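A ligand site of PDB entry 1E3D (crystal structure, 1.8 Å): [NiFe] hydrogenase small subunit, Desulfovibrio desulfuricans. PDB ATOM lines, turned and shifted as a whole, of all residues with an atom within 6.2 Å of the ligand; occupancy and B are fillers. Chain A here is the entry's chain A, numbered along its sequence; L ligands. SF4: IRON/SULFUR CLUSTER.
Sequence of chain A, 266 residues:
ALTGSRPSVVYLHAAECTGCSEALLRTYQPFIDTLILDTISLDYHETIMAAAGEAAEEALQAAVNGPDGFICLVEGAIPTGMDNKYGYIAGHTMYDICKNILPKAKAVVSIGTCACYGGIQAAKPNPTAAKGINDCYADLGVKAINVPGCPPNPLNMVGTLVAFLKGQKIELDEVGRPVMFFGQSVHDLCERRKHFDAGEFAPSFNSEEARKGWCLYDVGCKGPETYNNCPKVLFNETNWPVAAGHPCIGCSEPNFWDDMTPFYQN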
ATOM      1  N   VAL A 186      -7.416   3.377 -32.141  1.00  0.00           N
ATOM      2  CA  VAL A 186      -6.315   3.725 -31.262  1.00  0.00           C
ATOM      3  C   VAL A 186      -6.603   3.328 -29.815  1.00  0.00           C
ATOM      4  O   VAL A 186      -5.787   2.733 -29.111  1.00  0.00           O
ATOM      5  CB  VAL A 186      -6.084   5.248 -31.346  1.00  0.00           C
ATOM      6  CG1 VAL A 186      -5.230   5.739 -30.197  1.00  0.00           C
ATOM      7  CG2 VAL A 186      -5.449   5.605 -32.690  1.00  0.00           C
ATOM      8  N   HIS A 187      -7.789   3.663 -29.340  1.00  0.00           N
ATOM      9  CA  HIS A 187      -8.196   3.389 -27.963  1.00  0.00           C
ATOM     10  C   HIS A 187      -8.168   1.884 -27.684  1.00  0.00           C
ATOM     11  O   HIS A 187      -7.682   1.461 -26.630  1.00  0.00           O
ATOM     12  CB  HIS A 187      -9.587   3.971 -27.699  1.00  0.00           C
ATOM     13  CG  HIS A 187     -10.212   3.708 -26.363  1.00  0.00           C
ATOM     14  ND1 HIS A 187      -9.800   4.334 -25.207  1.00  0.00           N
ATOM     15  CD2 HIS A 187     -11.234   2.887 -25.985  1.00  0.00           C
ATOM     16  CE1 HIS A 187     -10.518   3.921 -24.184  1.00  0.00           C
ATOM     17  NE2 HIS A 187     -11.406   3.032 -24.627  1.00  0.00           N
ATOM     18  N   ASP A 188      -8.674   1.063 -28.604  1.00  0.00           N
ATOM     19  CA  ASP A 188      -8.644  -0.375 -28.291  1.00  0.00           C
ATOM     20  C   ASP A 188      -7.216  -0.864 -28.114  1.00  0.00           C
ATOM     21  O   ASP A 188      -6.979  -1.821 -27.365  1.00  0.00           O
ATOM     22  CB  ASP A 188      -9.379  -1.207 -29.345  1.00  0.00           C
ATOM     23  CG  ASP A 188     -10.889  -1.144 -29.227  1.00  0.00           C
ATOM     24  OD1 ASP A 188     -11.412  -0.654 -28.212  1.00  0.00           O
ATOM     25  OD2 ASP A 188     -11.586  -1.572 -30.174  1.00  0.00           O
ATOM     26  N   CYS A 190      -4.718   0.977 -26.965  1.00  0.00           N
ATOM     27  CA  CYS A 190      -4.008   1.830 -26.028  1.00  0.00           C
ATOM     28  C   CYS A 190      -3.657   1.122 -24.722  1.00  0.00           C
ATOM     29  O   CYS A 190      -4.538   0.493 -24.143  1.00  0.00           O
ATOM     30  CB  CYS A 190      -4.820   3.111 -25.738  1.00  0.00           C
ATOM     31  SG  CYS A 190      -3.962   4.275 -24.641  1.00  0.00           S
ATOM     32  N   GLU A 191      -2.418   1.274 -24.286  1.00  0.00           N
ATOM     33  CA  GLU A 191      -1.929   0.779 -23.015  1.00  0.00           C
ATOM     34  C   GLU A 191      -2.546   1.475 -21.815  1.00  0.00           C
ATOM     35  O   GLU A 191      -2.425   0.965 -20.691  1.00  0.00           O
ATOM     36  CB  GLU A 191      -0.394   0.873 -22.922  1.00  0.00           C
ATOM     37  CG  GLU A 191       0.179   2.282 -22.929  1.00  0.00           C
ATOM     38  CD  GLU A 191       0.548   2.764 -24.312  1.00  0.00           C
ATOM     39  OE1 GLU A 191      -0.057   2.270 -25.301  1.00  0.00           O
ATOM     40  OE2 GLU A 191       1.434   3.651 -24.409  1.00  0.00           O
ATOM     41  N   ARG A 192      -3.222   2.612 -21.964  1.00  0.00           N
ATOM     42  CA  ARG A 192      -3.854   3.223 -20.805  1.00  0.00           C
ATOM     43  C   ARG A 192      -5.343   2.863 -20.748  1.00  0.00           C
ATOM     44  O   ARG A 192      -6.036   3.456 -19.925  1.00  0.00           O
ATOM     45  CB  ARG A 192      -3.695   4.743 -20.775  1.00  0.00           C
ATOM     46  CG  ARG A 192      -2.273   5.242 -20.982  1.00  0.00           C
ATOM     47  CD  ARG A 192      -2.119   6.736 -20.738  1.00  0.00           C
ATOM     48  NE  ARG A 192      -0.707   7.104 -20.731  1.00  0.00           N
ATOM     49  CZ  ARG A 192      -0.183   8.246 -20.313  1.00  0.00           C
ATOM     50  NH1 ARG A 192      -0.936   9.227 -19.829  1.00  0.00           N
ATOM     51  NH2 ARG A 192       1.135   8.430 -20.370  1.00  0.00           N
ATOM     52  N   ARG A 193      -5.799   1.962 -21.596  1.00  0.00           N
ATOM     53  CA  ARG A 193      -7.209   1.566 -21.627  1.00  0.00           C
ATOM     54  C   ARG A 193      -7.662   1.020 -20.279  1.00  0.00           C
ATOM     55  O   ARG A 193      -8.794   1.228 -19.846  1.00  0.00           O
ATOM     56  CB  ARG A 193      -7.454   0.544 -22.751  1.00  0.00           C
ATOM     57  CG  ARG A 193      -8.930   0.334 -23.058  1.00  0.00           C
ATOM     58  CD  ARG A 193      -9.145  -0.779 -24.059  1.00  0.00           C
ATOM     59  NE  ARG A 193     -10.554  -0.882 -24.425  1.00  0.00           N
ATOM     60  CZ  ARG A 193     -11.095  -1.902 -25.103  1.00  0.00           C
ATOM     61  NH1 ARG A 193     -10.315  -2.898 -25.478  1.00  0.00           N
ATOM     62  NH2 ARG A 193     -12.391  -1.890 -25.393  1.00  0.00           N
ATOM     63  N   LYS A 194      -6.779   0.317 -19.567  1.00  0.00           N
ATOM     64  CA  LYS A 194      -7.140  -0.188 -18.246  1.00  0.00           C
ATOM     65  C   LYS A 194      -7.545   0.968 -17.345  1.00  0.00           C
ATOM     66  O   LYS A 194      -8.441   0.821 -16.522  1.00  0.00           O
ATOM     67  CB  LYS A 194      -6.006  -0.974 -17.577  1.00  0.00           C
ATOM     68  CG  LYS A 194      -4.899  -0.111 -16.993  1.00  0.00           C
ATOM     69  CD  LYS A 194      -3.624  -0.921 -16.861  1.00  0.00           C
ATOM     70  CE  LYS A 194      -2.378  -0.033 -16.911  1.00  0.00           C
ATOM     71  NZ  LYS A 194      -1.210  -0.682 -16.258  1.00  0.00           N
ATOM     72  N   HIS A 195      -6.894   2.118 -17.510  1.00  0.00           N
ATOM     73  CA  HIS A 195      -7.214   3.246 -16.633  1.00  0.00           C
ATOM     74  C   HIS A 195      -8.577   3.831 -17.007  1.00  0.00           C
ATOM     75  O   HIS A 195      -9.381   4.185 -16.165  1.00  0.00           O
ATOM     76  CB  HIS A 195      -6.126   4.307 -16.693  1.00  0.00           C
ATOM     77  CG  HIS A 195      -4.796   3.880 -16.156  1.00  0.00           C
ATOM     78  ND1 HIS A 195      -4.607   3.574 -14.818  1.00  0.00           N
ATOM     79  CD2 HIS A 195      -3.593   3.724 -16.740  1.00  0.00           C
ATOM     80  CE1 HIS A 195      -3.355   3.238 -14.620  1.00  0.00           C
ATOM     81  NE2 HIS A 195      -2.707   3.316 -15.766  1.00  0.00           N
ATOM     82  N   PHE A 196      -8.817   3.928 -18.304  1.00  0.00           N
ATOM     83  CA  PHE A 196     -10.104   4.396 -18.816  1.00  0.00           C
ATOM     84  C   PHE A 196     -11.256   3.620 -18.175  1.00  0.00           C
ATOM     85  O   PHE A 196     -12.234   4.176 -17.660  1.00  0.00           O
ATOM     86  CB  PHE A 196     -10.123   4.233 -20.331  1.00  0.00           C
ATOM     87  CG  PHE A 196     -11.368   4.678 -21.075  1.00  0.00           C
ATOM     88  CD1 PHE A 196     -12.435   3.807 -21.241  1.00  0.00           C
ATOM     89  CD2 PHE A 196     -11.473   5.941 -21.606  1.00  0.00           C
ATOM     90  CE1 PHE A 196     -13.571   4.177 -21.931  1.00  0.00           C
ATOM     91  CE2 PHE A 196     -12.614   6.323 -22.301  1.00  0.00           C
ATOM     92  CZ  PHE A 196     -13.659   5.447 -22.464  1.00  0.00           C
ATOM     93  N   PHE A 201      -8.646   9.046 -14.627  1.00  0.00           N
ATOM     94  CA  PHE A 201      -8.372  10.080 -15.615  1.00  0.00           C
ATOM     95  C   PHE A 201      -7.494  11.211 -15.093  1.00  0.00           C
ATOM     96  O   PHE A 201      -7.613  11.602 -13.924  1.00  0.00           O
ATOM     97  CB  PHE A 201      -9.685  10.714 -16.123  1.00  0.00           C
ATOM     98  CG  PHE A 201     -10.688   9.720 -16.677  1.00  0.00           C
ATOM     99  CD1 PHE A 201     -10.517   9.169 -17.918  1.00  0.00           C
ATOM    100  CD2 PHE A 201     -11.811   9.337 -15.943  1.00  0.00           C
ATOM    101  CE1 PHE A 201     -11.396   8.255 -18.465  1.00  0.00           C
ATOM    102  CE2 PHE A 201     -12.698   8.420 -16.467  1.00  0.00           C
ATOM    103  CZ  PHE A 201     -12.508   7.866 -17.719  1.00  0.00           C
ATOM    104  N   TRP A 214      -2.160   8.228 -16.186  1.00  0.00           N
ATOM    105  CA  TRP A 214      -3.587   7.857 -16.356  1.00  0.00           C
ATOM    106  C   TRP A 214      -4.158   8.319 -17.689  1.00  0.00           C
ATOM    107  O   TRP A 214      -3.499   8.965 -18.502  1.00  0.00           O
ATOM    108  CB  TRP A 214      -4.397   8.389 -15.181  1.00  0.00           C
ATOM    109  CG  TRP A 214      -4.208   7.563 -13.944  1.00  0.00           C
ATOM    110  CD1 TRP A 214      -3.315   6.541 -13.793  1.00  0.00           C
ATOM    111  CD2 TRP A 214      -4.902   7.682 -12.700  1.00  0.00           C
ATOM    112  NE1 TRP A 214      -3.413   6.013 -12.526  1.00  0.00           N
ATOM    113  CE2 TRP A 214      -4.382   6.692 -11.836  1.00  0.00           C
ATOM    114  CE3 TRP A 214      -5.913   8.525 -12.227  1.00  0.00           C
ATOM    115  CZ2 TRP A 214      -4.841   6.532 -10.526  1.00  0.00           C
ATOM    116  CZ3 TRP A 214      -6.368   8.354 -10.926  1.00  0.00           C
ATOM    117  CH2 TRP A 214      -5.838   7.373 -10.092  1.00  0.00           C
ATOM    118  N   CYS A 215      -5.408   7.935 -17.948  1.00  0.00           N
ATOM    119  CA  CYS A 215      -6.046   8.122 -19.234  1.00  0.00           C
ATOM    120  C   CYS A 215      -6.228   9.605 -19.546  1.00  0.00           C
ATOM    121  O   CYS A 215      -6.430  10.386 -18.611  1.00  0.00           O
ATOM    122  CB  CYS A 215      -7.381   7.379 -19.293  1.00  0.00           C
ATOM    123  SG  CYS A 215      -8.402   7.770 -20.713  1.00  0.00           S
ATOM    124  N   LEU A 216      -6.149   9.970 -20.817  1.00  0.00           N
ATOM    125  CA  LEU A 216      -6.134  11.369 -21.248  1.00  0.00           C
ATOM    126  C   LEU A 216      -7.468  11.850 -21.794  1.00  0.00           C
ATOM    127  O   LEU A 216      -7.608  12.951 -22.347  1.00  0.00           O
ATOM    128  CB  LEU A 216      -5.011  11.588 -22.277  1.00  0.00           C
ATOM    129  CG  LEU A 216      -3.598  11.249 -21.782  1.00  0.00           C
ATOM    130  CD1 LEU A 216      -2.558  11.594 -22.837  1.00  0.00           C
ATOM    131  CD2 LEU A 216      -3.286  11.966 -20.465  1.00  0.00           C
ATOM    132  N   TYR A 217      -8.512  11.029 -21.621  1.00  0.00           N
ATOM    133  CA  TYR A 217      -9.806  11.351 -22.188  1.00  0.00           C
ATOM    134  C   TYR A 217     -10.332  12.714 -21.760  1.00  0.00           C
ATOM    135  O   TYR A 217     -10.929  13.446 -22.568  1.00  0.00           O
ATOM    136  CB  TYR A 217     -10.850  10.285 -21.805  1.00  0.00           C
ATOM    137  CG  TYR A 217     -12.164  10.482 -22.537  1.00  0.00           C
ATOM    138  CD1 TYR A 217     -12.334  10.043 -23.841  1.00  0.00           C
ATOM    139  CD2 TYR A 217     -13.244  11.104 -21.912  1.00  0.00           C
ATOM    140  CE1 TYR A 217     -13.537  10.221 -24.507  1.00  0.00           C
ATOM    141  CE2 TYR A 217     -14.436  11.276 -22.566  1.00  0.00           C
ATOM    142  CZ  TYR A 217     -14.593  10.837 -23.865  1.00  0.00           C
ATOM    143  OH  TYR A 217     -15.788  11.011 -24.533  1.00  0.00           O
ATOM    144  N   CYS A 221      -8.524  13.426 -25.318  1.00  0.00           N
ATOM    145  CA  CYS A 221      -8.136  12.330 -26.196  1.00  0.00           C
ATOM    146  C   CYS A 221      -9.267  11.743 -27.025  1.00  0.00           C
ATOM    147  O   CYS A 221     -10.379  11.396 -26.606  1.00  0.00           O
ATOM    148  CB  CYS A 221      -7.446  11.224 -25.377  1.00  0.00           C
ATOM    149  SG  CYS A 221      -6.751   9.917 -26.383  1.00  0.00           S
ATOM    150  N   LYS A 222      -8.981  11.628 -28.328  1.00  0.00           N
ATOM    151  CA  LYS A 222      -9.950  11.210 -29.336  1.00  0.00           C
ATOM    152  C   LYS A 222      -9.711   9.776 -29.764  1.00  0.00           C
ATOM    153  O   LYS A 222     -10.342   9.316 -30.704  1.00  0.00           O
ATOM    154  CB  LYS A 222      -9.929  12.121 -30.573  1.00  0.00           C
ATOM    155  CG  LYS A 222     -10.206  13.585 -30.287  1.00  0.00           C
ATOM    156  CD  LYS A 222     -11.362  13.770 -29.305  1.00  0.00           C
ATOM    157  CE  LYS A 222     -11.896  15.195 -29.360  1.00  0.00           C
ATOM    158  NZ  LYS A 222     -10.974  16.160 -28.708  1.00  0.00           N
ATOM    159  N   GLY A 223      -8.805   9.099 -29.076  1.00  0.00           N
ATOM    160  CA  GLY A 223      -8.488   7.704 -29.269  1.00  0.00           C
ATOM    161  C   GLY A 223      -9.691   6.824 -29.535  1.00  0.00           C
ATOM    162  O   GLY A 223      -9.672   6.017 -30.463  1.00  0.00           O
ATOM    163  N   PRO A 224     -10.732   6.942 -28.715  1.00  0.00           N
ATOM    164  CA  PRO A 224     -11.948   6.146 -28.950  1.00  0.00           C
ATOM    165  C   PRO A 224     -12.679   6.400 -30.251  1.00  0.00           C
ATOM    166  O   PRO A 224     -13.459   5.535 -30.659  1.00  0.00           O
ATOM    167  CB  PRO A 224     -12.857   6.556 -27.767  1.00  0.00           C
ATOM    168  CG  PRO A 224     -11.919   7.044 -26.720  1.00  0.00           C
ATOM    169  CD  PRO A 224     -10.836   7.751 -27.477  1.00  0.00           C
ATOM    170  N   TRP A 240       4.584   7.094 -29.065  1.00  0.00           N
ATOM    171  CA  TRP A 240       3.375   7.636 -29.706  1.00  0.00           C
ATOM    172  C   TRP A 240       2.786   8.723 -28.838  1.00  0.00           C
ATOM    173  O   TRP A 240       3.224   8.899 -27.696  1.00  0.00           O
ATOM    174  CB  TRP A 240       2.429   6.517 -30.086  1.00  0.00           C
ATOM    175  CG  TRP A 240       1.701   5.862 -28.967  1.00  0.00           C
ATOM    176  CD1 TRP A 240       2.187   5.063 -27.980  1.00  0.00           C
ATOM    177  CD2 TRP A 240       0.286   5.960 -28.740  1.00  0.00           C
ATOM    178  NE1 TRP A 240       1.169   4.658 -27.143  1.00  0.00           N
ATOM    179  CE2 TRP A 240      -0.013   5.195 -27.595  1.00  0.00           C
ATOM    180  CE3 TRP A 240      -0.754   6.621 -29.393  1.00  0.00           C
ATOM    181  CZ2 TRP A 240      -1.308   5.082 -27.097  1.00  0.00           C
ATOM    182  CZ3 TRP A 240      -2.034   6.514 -28.897  1.00  0.00           C
ATOM    183  CH2 TRP A 240      -2.311   5.744 -27.749  1.00  0.00           C
ATOM    184  N   VAL A 242       0.144   9.448 -26.932  1.00  0.00           N
ATOM    185  CA  VAL A 242      -0.370   9.257 -25.572  1.00  0.00           C
ATOM    186  C   VAL A 242       0.754   8.817 -24.627  1.00  0.00           C
ATOM    187  O   VAL A 242       0.787   9.181 -23.458  1.00  0.00           O
ATOM    188  CB  VAL A 242      -1.497   8.236 -25.532  1.00  0.00           C
ATOM    189  CG1 VAL A 242      -1.746   7.789 -24.088  1.00  0.00           C
ATOM    190  CG2 VAL A 242      -2.756   8.843 -26.145  1.00  0.00           C
ATOM    191  N   PRO A 247      -2.867  13.880 -25.557  1.00  0.00           N
ATOM    192  CA  PRO A 247      -3.992  13.193 -26.179  1.00  0.00           C
ATOM    193  C   PRO A 247      -3.839  13.073 -27.691  1.00  0.00           C
ATOM    194  O   PRO A 247      -3.141  13.866 -28.311  1.00  0.00           O
ATOM    195  CB  PRO A 247      -5.174  14.105 -25.858  1.00  0.00           C
ATOM    196  CG  PRO A 247      -4.600  15.416 -25.420  1.00  0.00           C
ATOM    197  CD  PRO A 247      -3.241  15.129 -24.884  1.00  0.00           C
ATOM    198  N   CYS A 248      -4.502  12.058 -28.225  1.00  0.00           N
ATOM    199  CA  CYS A 248      -4.708  11.831 -29.642  1.00  0.00           C
ATOM    200  C   CYS A 248      -5.625  12.943 -30.155  1.00  0.00           C
ATOM    201  O   CYS A 248      -6.605  13.336 -29.509  1.00  0.00           O
ATOM    202  CB  CYS A 248      -5.298  10.450 -29.896  1.00  0.00           C
ATOM    203  SG  CYS A 248      -5.806  10.089 -31.589  1.00  0.00           S
ATOM    204  N   ASN A 266     -13.315  16.775 -24.336  1.00  0.00           N
ATOM    205  CA  ASN A 266     -14.222  15.771 -24.864  1.00  0.00           C
ATOM    206  C   ASN A 266     -15.660  16.128 -24.446  1.00  0.00           C
ATOM    207  O   ASN A 266     -15.820  17.063 -23.649  1.00  0.00           O
ATOM    208  CB  ASN A 266     -13.886  14.353 -24.422  1.00  0.00           C
ATOM    209  CG  ASN A 266     -13.093  13.568 -25.444  1.00  0.00           C
ATOM    210  OD1 ASN A 266     -13.539  13.314 -26.563  1.00  0.00           O
ATOM    211  ND2 ASN A 266     -11.878  13.167 -25.065  1.00  0.00           N
ATOM    212  OXT ASN A 266     -16.590  15.457 -24.942  1.00  0.00           O
HETATM  213 FE1  SF4 L   1      -6.928   7.986 -25.177  1.00  0.00          FE
HETATM  214 FE2  SF4 L   1      -5.723   5.759 -24.268  1.00  0.00          FE
HETATM  215 FE3  SF4 L   1      -7.553   6.971 -22.688  1.00  0.00          FE
HETATM  216 FE4  SF4 L   1      -8.389   5.754 -24.830  1.00  0.00          FE
HETATM  217  S1  SF4 L   1      -7.369   4.757 -22.943  1.00  0.00           S
HETATM  218  S2  SF4 L   1      -8.992   7.838 -24.199  1.00  0.00           S
HETATM  219  S3  SF4 L   1      -6.657   6.072 -26.378  1.00  0.00           S
HETATM  220  S4  SF4 L   1      -5.415   7.747 -23.324  1.00  0.00           S
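The backbone NH (N) of Leu 216 sits close to a sulfur (S4) of the ligand (3.4 Å). An iron atom (FE4) of the ligand is bound by a ring nitrogen (ND1) of His 187 (2.0 Å). The side-chain sulfur of Cys 190 is bound to an iron atom (FE2) of the ligand, 2.3 Å away. An iron atom (FE1) of the ligand is bound by the side-chain sulfur (SG) of Cys 221, 2.3 Å away. S1 of the ligand lies close to N of Arg 193 (3.5 Å). SG of Cys 215 binds FE3 of the ligand (2.3 Å).
The side-chain sulfur (SG) of Cys 215 sits close to the backbone NH (N) of Tyr 217. NH2 of Arg 193 is in salt-bridge range of OD1 of Asp 188. The side-chain sulfur of Cys 190 lies close to the backbone NH of Arg 192 (3.2 Å). The backbone carbonyl oxygen (O) of Gly 223 is in hydrogen-bond range of the backbone NH (N) of His 187 (3.2 Å). The side-chain amide nitrogen (ND2) of Asn 266 is in hydrogen-bond range of the backbone carbonyl oxygen (O) of Cys 221, 2.8 Å away. NH2 of Arg 192 sits at hydrogen-bond distance from O of Val 242 (3.2 Å). The side-chain sulfur (SG) of Cys 221 lies close to the backbone NH (N) of Cys 248, at 3.6 Å. O of Leu 216 lies within hydrogen-bond range of N of Cys 221 (3.1 Å).
A sulfur (S1) of the ligand lies close to the backbone carbonyl oxygen of Arg 192 (3.5 Å). CB of Phe 196 touches S1 of the ligand, at 3.8 Å. Tyr 217 touches the ligand. Gly 223 touches the ligand. Pro 224 touches the ligand. CG1 of Val 242 touches S4 of the ligand, 3.7 Å away. Hydrophobic or aromatic side chains that line the ligand: His 187, Phe 196, Tyr 217, Pro 224 and Val 242. Of the 24 residues printed, 12 come within 4 Å of the ligand.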
